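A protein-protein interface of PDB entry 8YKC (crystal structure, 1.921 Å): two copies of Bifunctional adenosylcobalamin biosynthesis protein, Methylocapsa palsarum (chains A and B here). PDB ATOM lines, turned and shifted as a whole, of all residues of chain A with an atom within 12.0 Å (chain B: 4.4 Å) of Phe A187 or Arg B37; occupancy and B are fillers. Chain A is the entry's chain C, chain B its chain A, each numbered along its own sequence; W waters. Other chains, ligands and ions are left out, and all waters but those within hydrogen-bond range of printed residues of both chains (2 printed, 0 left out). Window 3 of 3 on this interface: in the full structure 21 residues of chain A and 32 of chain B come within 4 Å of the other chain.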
ATOM      1  N   PRO A 183       0.105  12.908   9.774  1.00  0.00           N
ATOM      2  CA  PRO A 183       0.343  12.172   8.537  1.00  0.00           C
ATOM      3  C   PRO A 183       1.442  11.142   8.803  1.00  0.00           C
ATOM      4  O   PRO A 183       2.221  11.318   9.742  1.00  0.00           O
ATOM      5  CB  PRO A 183       0.756  13.262   7.533  1.00  0.00           C
ATOM      6  CG  PRO A 183       1.375  14.317   8.408  1.00  0.00           C
ATOM      7  CD  PRO A 183       0.543  14.312   9.673  1.00  0.00           C
ATOM      8  N   VAL A 184       1.418  10.075   8.005  1.00  0.00           N
ATOM      9  CA  VAL A 184       2.377   8.948   8.005  1.00  0.00           C
ATOM     10  C   VAL A 184       2.811   8.763   6.549  1.00  0.00           C
ATOM     11  O   VAL A 184       1.987   8.931   5.636  1.00  0.00           O
ATOM     12  CB  VAL A 184       1.752   7.694   8.653  1.00  0.00           C
ATOM     13  CG1 VAL A 184       2.598   6.443   8.431  1.00  0.00           C
ATOM     14  CG2 VAL A 184       1.531   7.935  10.133  1.00  0.00           C
ATOM     15  N   PHE A 185       4.108   8.579   6.354  1.00  0.00           N
ATOM     16  CA  PHE A 185       4.746   8.362   5.032  1.00  0.00           C
ATOM     17  C   PHE A 185       5.504   7.039   5.100  1.00  0.00           C
ATOM     18  O   PHE A 185       6.142   6.777   6.116  1.00  0.00           O
ATOM     19  CB  PHE A 185       5.659   9.540   4.706  1.00  0.00           C
ATOM     20  CG  PHE A 185       4.902  10.829   4.659  1.00  0.00           C
ATOM     21  CD1 PHE A 185       4.005  11.062   3.641  1.00  0.00           C
ATOM     22  CD2 PHE A 185       4.998  11.735   5.699  1.00  0.00           C
ATOM     23  CE1 PHE A 185       3.281  12.242   3.612  1.00  0.00           C
ATOM     24  CE2 PHE A 185       4.267  12.909   5.672  1.00  0.00           C
ATOM     25  CZ  PHE A 185       3.406  13.155   4.630  1.00  0.00           C
ATOM     26  N   ARG A 186       5.367   6.208   4.077  1.00  0.00           N
ATOM     27  CA  ARG A 186       5.999   4.876   4.027  1.00  0.00           C
ATOM     28  C   ARG A 186       7.117   4.858   2.976  1.00  0.00           C
ATOM     29  O   ARG A 186       6.937   5.489   1.909  1.00  0.00           O
ATOM     30  CB  ARG A 186       4.885   3.852   3.814  1.00  0.00           C
ATOM     31  CG  ARG A 186       4.065   3.692   5.087  1.00  0.00           C
ATOM     32  CD  ARG A 186       3.073   2.559   5.048  1.00  0.00           C
ATOM     33  NE  ARG A 186       3.585   1.209   5.254  1.00  0.00           N
ATOM     34  CZ  ARG A 186       3.821   0.320   4.290  1.00  0.00           C
ATOM     35  NH1 ARG A 186       3.667   0.630   3.013  1.00  0.00           N
ATOM     36  NH2 ARG A 186       4.243  -0.889   4.612  1.00  0.00           N
ATOM     37  N   PHE A 187       8.205   4.128   3.262  1.00  0.00           N
ATOM     38  CA  PHE A 187       9.388   4.046   2.369  1.00  0.00           C
ATOM     39  C   PHE A 187       9.780   2.580   2.115  1.00  0.00           C
ATOM     40  O   PHE A 187      10.718   2.495   1.273  1.00  0.00           O
ATOM     41  CB  PHE A 187      10.561   4.845   2.946  1.00  0.00           C
ATOM     42  CG  PHE A 187      10.227   6.263   3.348  1.00  0.00           C
ATOM     43  CD1 PHE A 187       9.762   6.542   4.620  1.00  0.00           C
ATOM     44  CD2 PHE A 187      10.356   7.313   2.451  1.00  0.00           C
ATOM     45  CE1 PHE A 187       9.505   7.852   5.012  1.00  0.00           C
ATOM     46  CE2 PHE A 187      10.048   8.614   2.827  1.00  0.00           C
ATOM     47  CZ  PHE A 187       9.627   8.884   4.108  1.00  0.00           C
ATOM     48  N   PRO B  10       4.767   3.098  -0.898  1.00  0.00           N
ATOM     49  CA  PRO B  10       6.100   3.661  -0.698  1.00  0.00           C
ATOM     50  C   PRO B  10       6.314   4.920  -1.543  1.00  0.00           C
ATOM     51  O   PRO B  10       5.932   4.907  -2.684  1.00  0.00           O
ATOM     52  CB  PRO B  10       7.022   2.503  -1.107  1.00  0.00           C
ATOM     53  CG  PRO B  10       6.238   1.268  -0.741  1.00  0.00           C
ATOM     54  CD  PRO B  10       4.794   1.632  -1.036  1.00  0.00           C
ATOM     55  N   ILE B  11       6.879   5.991  -0.949  1.00  0.00           N
ATOM     56  CA  ILE B  11       7.350   7.190  -1.709  1.00  0.00           C
ATOM     57  C   ILE B  11       8.888   7.185  -1.736  1.00  0.00           C
ATOM     58  O   ILE B  11       9.547   6.433  -0.937  1.00  0.00           O
ATOM     59  CB  ILE B  11       6.800   8.501  -1.098  1.00  0.00           C
ATOM     60  CG1 ILE B  11       7.317   8.705   0.332  1.00  0.00           C
ATOM     61  CG2 ILE B  11       5.287   8.543  -1.164  1.00  0.00           C
ATOM     62  CD1 ILE B  11       6.947  10.013   0.960  1.00  0.00           C
ATOM     63  N   LEU B  14      10.618  12.881   0.859  1.00  0.00           N
ATOM     64  CA  LEU B  14       9.794  13.675   1.792  1.00  0.00           C
ATOM     65  C   LEU B  14      10.595  14.909   2.183  1.00  0.00           C
ATOM     66  O   LEU B  14      11.772  14.760   2.557  1.00  0.00           O
ATOM     67  CB  LEU B  14       9.458  12.813   3.004  1.00  0.00           C
ATOM     68  CG  LEU B  14       8.823  13.559   4.182  1.00  0.00           C
ATOM     69  CD1 LEU B  14       7.494  14.170   3.782  1.00  0.00           C
ATOM     70  CD2 LEU B  14       8.657  12.626   5.358  1.00  0.00           C
ATOM     71  N   MET B  31       9.371   8.862  11.231  1.00  0.00           N
ATOM     72  CA  MET B  31       9.004   8.336   9.895  1.00  0.00           C
ATOM     73  C   MET B  31      10.051   7.297   9.467  1.00  0.00           C
ATOM     74  O   MET B  31       9.646   6.228   9.015  1.00  0.00           O
ATOM     75  CB  MET B  31       8.891   9.440   8.843  1.00  0.00           C
ATOM     76  CG  MET B  31       7.662  10.333   8.962  1.00  0.00           C
ATOM     77  SD  MET B  31       6.060   9.449   9.157  1.00  0.00           S
ATOM     78  CE  MET B  31       5.886   9.443  10.937  1.00  0.00           C
ATOM     79  N   SER B  35      10.046   2.624   9.070  1.00  0.00           N
ATOM     80  CA  SER B  35      10.395   1.874   7.833  1.00  0.00           C
ATOM     81  C   SER B  35      11.198   0.607   8.194  1.00  0.00           C
ATOM     82  O   SER B  35      11.691   0.489   9.326  1.00  0.00           O
ATOM     83  CB  SER B  35      11.151   2.772   6.870  1.00  0.00           C
ATOM     84  OG  SER B  35      12.562   2.763   7.161  1.00  0.00           O
ATOM     85  N   GLY B  36      11.397  -0.293   7.241  1.00  0.00           N
ATOM     86  CA  GLY B  36      12.309  -1.445   7.410  1.00  0.00           C
ATOM     87  C   GLY B  36      13.665  -1.244   6.748  1.00  0.00           C
ATOM     88  O   GLY B  36      14.359  -2.264   6.518  1.00  0.00           O
ATOM     89  N   ARG B  37      14.078   0.013   6.484  1.00  0.00           N
ATOM     90  CA  ARG B  37      15.317   0.302   5.719  1.00  0.00           C
ATOM     91  C   ARG B  37      16.501   0.439   6.690  1.00  0.00           C
ATOM     92  O   ARG B  37      16.282   0.691   7.874  1.00  0.00           O
ATOM     93  CB  ARG B  37      15.174   1.554   4.849  1.00  0.00           C
ATOM     94  CG  ARG B  37      13.923   1.598   3.982  1.00  0.00           C
ATOM     95  CD  ARG B  37      14.074   0.719   2.753  1.00  0.00           C
ATOM     96  NE  ARG B  37      12.830   0.585   2.013  1.00  0.00           N
ATOM     97  CZ  ARG B  37      12.468  -0.504   1.310  1.00  0.00           C
ATOM     98  NH1 ARG B  37      13.247  -1.579   1.265  1.00  0.00           N
ATOM     99  NH2 ARG B  37      11.310  -0.521   0.670  1.00  0.00           N
ATOM    100  N   SER B  38      17.724   0.226   6.193  1.00  0.00           N
ATOM    101  CA  SER B  38      18.966   0.666   6.869  1.00  0.00           C
ATOM    102  C   SER B  38      18.969   2.193   6.982  1.00  0.00           C
ATOM    103  O   SER B  38      18.958   2.874   5.923  1.00  0.00           O
ATOM    104  CB  SER B  38      20.162   0.135   6.132  1.00  0.00           C
ATOM    105  OG  SER B  38      19.931  -1.246   5.920  1.00  0.00           O
ATOM    106  N   LEU B  39      18.924   2.704   8.212  1.00  0.00           N
ATOM    107  CA  LEU B  39      18.737   4.150   8.500  1.00  0.00           C
ATOM    108  C   LEU B  39      20.100   4.827   8.523  1.00  0.00           C
ATOM    109  O   LEU B  39      20.980   4.354   9.280  1.00  0.00           O
ATOM    110  CB  LEU B  39      17.967   4.305   9.814  1.00  0.00           C
ATOM    111  CG  LEU B  39      16.621   3.595   9.821  1.00  0.00           C
ATOM    112  CD1 LEU B  39      15.853   3.923  11.081  1.00  0.00           C
ATOM    113  CD2 LEU B  39      15.821   3.949   8.573  1.00  0.00           C
ATOM    114  N   PRO B  86      18.323   1.243  -2.591  1.00  0.00           N
ATOM    115  CA  PRO B  86      16.947   0.808  -2.338  1.00  0.00           C
ATOM    116  C   PRO B  86      16.724   0.270  -0.914  1.00  0.00           C
ATOM    117  O   PRO B  86      15.630   0.391  -0.403  1.00  0.00           O
ATOM    118  CB  PRO B  86      16.698  -0.293  -3.402  1.00  0.00           C
ATOM    119  CG  PRO B  86      17.783  -0.094  -4.452  1.00  0.00           C
ATOM    120  CD  PRO B  86      18.954   0.527  -3.723  1.00  0.00           C
ATOM    121  N   GLU B  87      17.755  -0.284  -0.271  1.00  0.00           N
ATOM    122  CA  GLU B  87      17.615  -0.901   1.081  1.00  0.00           C
ATOM    123  C   GLU B  87      17.919   0.138   2.160  1.00  0.00           C
ATOM    124  O   GLU B  87      17.818  -0.202   3.312  1.00  0.00           O
ATOM    125  CB  GLU B  87      18.552  -2.095   1.309  1.00  0.00           C
ATOM    126  CG  GLU B  87      19.906  -1.979   0.645  1.00  0.00           C
ATOM    127  CD  GLU B  87      19.871  -2.390  -0.818  1.00  0.00           C
ATOM    128  OE1 GLU B  87      19.467  -3.541  -1.115  1.00  0.00           O
ATOM    129  OE2 GLU B  87      20.181  -1.551  -1.664  1.00  0.00           O
ATOM    130  N   ARG B  88      18.308   1.345   1.774  1.00  0.00           N
ATOM    131  CA  ARG B  88      18.632   2.428   2.726  1.00  0.00           C
ATOM    132  C   ARG B  88      17.566   3.519   2.721  1.00  0.00           C
ATOM    133  O   ARG B  88      16.914   3.751   1.675  1.00  0.00           O
ATOM    134  CB  ARG B  88      19.932   3.112   2.321  1.00  0.00           C
ATOM    135  CG  ARG B  88      21.167   2.431   2.863  1.00  0.00           C
ATOM    136  CD  ARG B  88      22.393   3.073   2.288  1.00  0.00           C
ATOM    137  NE  ARG B  88      23.572   2.738   3.048  1.00  0.00           N
ATOM    138  CZ  ARG B  88      24.758   3.293   2.859  1.00  0.00           C
ATOM    139  NH1 ARG B  88      24.942   4.227   1.944  1.00  0.00           N
ATOM    140  NH2 ARG B  88      25.759   2.933   3.619  1.00  0.00           N
ATOM    141  N   LEU B  89      17.486   4.228   3.841  1.00  0.00           N
ATOM    142  CA  LEU B  89      16.757   5.499   3.964  1.00  0.00           C
ATOM    143  C   LEU B  89      17.741   6.536   4.513  1.00  0.00           C
ATOM    144  O   LEU B  89      18.238   6.317   5.613  1.00  0.00           O
ATOM    145  CB  LEU B  89      15.537   5.312   4.854  1.00  0.00           C
ATOM    146  CG  LEU B  89      14.464   6.380   4.662  1.00  0.00           C
ATOM    147  CD1 LEU B  89      13.328   6.232   5.668  1.00  0.00           C
ATOM    148  CD2 LEU B  89      15.067   7.740   4.787  1.00  0.00           C
ATOM    149  N   PRO B 126      15.288   5.987  -1.123  1.00  0.00           N
ATOM    150  CA  PRO B 126      14.494   7.052  -0.514  1.00  0.00           C
ATOM    151  C   PRO B 126      15.285   7.966   0.424  1.00  0.00           C
ATOM    152  O   PRO B 126      16.328   7.542   0.967  1.00  0.00           O
ATOM    153  CB  PRO B 126      13.396   6.305   0.249  1.00  0.00           C
ATOM    154  CG  PRO B 126      14.023   4.980   0.583  1.00  0.00           C
ATOM    155  CD  PRO B 126      14.953   4.664  -0.573  1.00  0.00           C
ATOM    156  N   ILE B 128      14.725  11.608   3.158  1.00  0.00           N
ATOM    157  CA  ILE B 128      13.959  12.654   3.864  1.00  0.00           C
ATOM    158  C   ILE B 128      14.862  13.864   4.026  1.00  0.00           C
ATOM    159  O   ILE B 128      16.017  13.668   4.504  1.00  0.00           O
ATOM    160  CB  ILE B 128      13.437  12.145   5.210  1.00  0.00           C
ATOM    161  CG1 ILE B 128      12.548  10.910   5.022  1.00  0.00           C
ATOM    162  CG2 ILE B 128      12.699  13.280   5.919  1.00  0.00           C
ATOM    163  CD1 ILE B 128      12.137  10.222   6.298  1.00  0.00           C
HETATM  164  O   HOH W   1      10.969   4.215  -1.377  1.00  0.00           O
HETATM  165  O   HOH W   2       7.648   5.068   7.646  1.00  0.00           O
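SD of Met B31 is in hydrogen-bond range of N of Phe A185 (3.5 Å).
The guanidinium group (NE) of Arg B37 lies within hydrogen-bond range of the backbone carbonyl oxygen (O) of Phe A187 (2.9 Å).
The backbone NH of Ile B11 is in hydrogen-bond range of the backbone carbonyl oxygen of Arg A186, 2.9 Å away.
The side-chain hydroxyl (OG) of Ser B35 is in hydrogen-bond range of the backbone NH (N) of Arg B37.
O of Ser B38 lies within hydrogen-bond range of N of Leu B89.
Among the printed residues, pairs that only touch across the chains: Val A184 with Met B31 (3.9 Å), Phe A185 with Ile B11 (3.99 Å), Phe A185 with Leu B14 (3.8 Å), Arg A186 with Pro B10 (3.3 Å), Phe A187 with Ile B11 (3.6 Å), Phe A187 with Leu B89 (3.7 Å), Phe A187 with Pro B126 (3.9 Å) and Phe A187 with Ile B128 (3.6 Å).
Of chain A, only Phe A187 (2.9 Å) comes within 4 Å of Arg B37.
Of chain A, only Arg A186 comes within 4 Å of Pro B10.
Of chain A, only Phe A185 (3.8 Å) comes within 4 Å of Leu B14.
Of chain A, only Val A184 (3.9 Å) and Phe A185 (3.5 Å) come within 4 Å of Met B31.
No residue of chain A comes within 4 Å of Ser B35.
No residue of chain A comes within 4 Å of Ser B38.
No residue of chain A comes within 4 Å of Pro B86.
No residue of chain A comes within 4 Å of Glu B87.
Of chain A, only Phe A187 (3.7 Å) comes within 4 Å of Leu B89.
Pro B126 touches just one residue of chain A: Phe A187.
Printed residues of chain B within 4 Å of Arg A186: Pro B10 and Ile B11.
Printed residues of chain A within 4 Å of Ile B128: Phe A187 (3.6 Å).
Of the printed residues of chain B, Val A184 touches Met B31 (3.9 Å).
Of the printed residues of chain A, Ile B11 touches Phe A185 (3.99 Å), Arg A186 (2.9 Å) and Phe A187 (3.6 Å).
Printed residues of chain B within 4 Å of Phe A185: Ile B11, Leu B14 and Met B31.
The nearest residue of chain B that does not touch Phe A187 is Leu B14 (4.1 Å).
The nearest residue of chain A that does not touch Arg B37 is Arg A186 (7.2 Å).
The nearest printed residue of chain B that does not touch Arg A186 is Ser B35 (6.0 Å).
Printed residues of chain B that touch a printed residue of chain A: Pro B10, Ile B11, Leu B14, Met B31, Arg B37, Leu B89, Pro B126 and Ile B128.
Printed residues of chain A that touch a printed residue of chain B: Val A184, Phe A185, Arg A186 and Phe A187.
Among the printed residues, 11 pairs touch across the chains.
Among the printed residues, no Asp or Glu carboxylate lies within 4 Å of a Lys or Arg side-chain nitrogen of the other chain.
No position is printed for both chains.
Water W1 lies within hydrogen-bond range of the backbone carbonyl oxygen of Ile B11 (2.7 Å) and the backbone carbonyl oxygen of Phe A187 (3.2 Å).
Water W2 bridges the backbone carbonyl oxygen of Met B31 (2.7 Å) and the backbone carbonyl oxygen of Phe A185 (2.7 Å).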
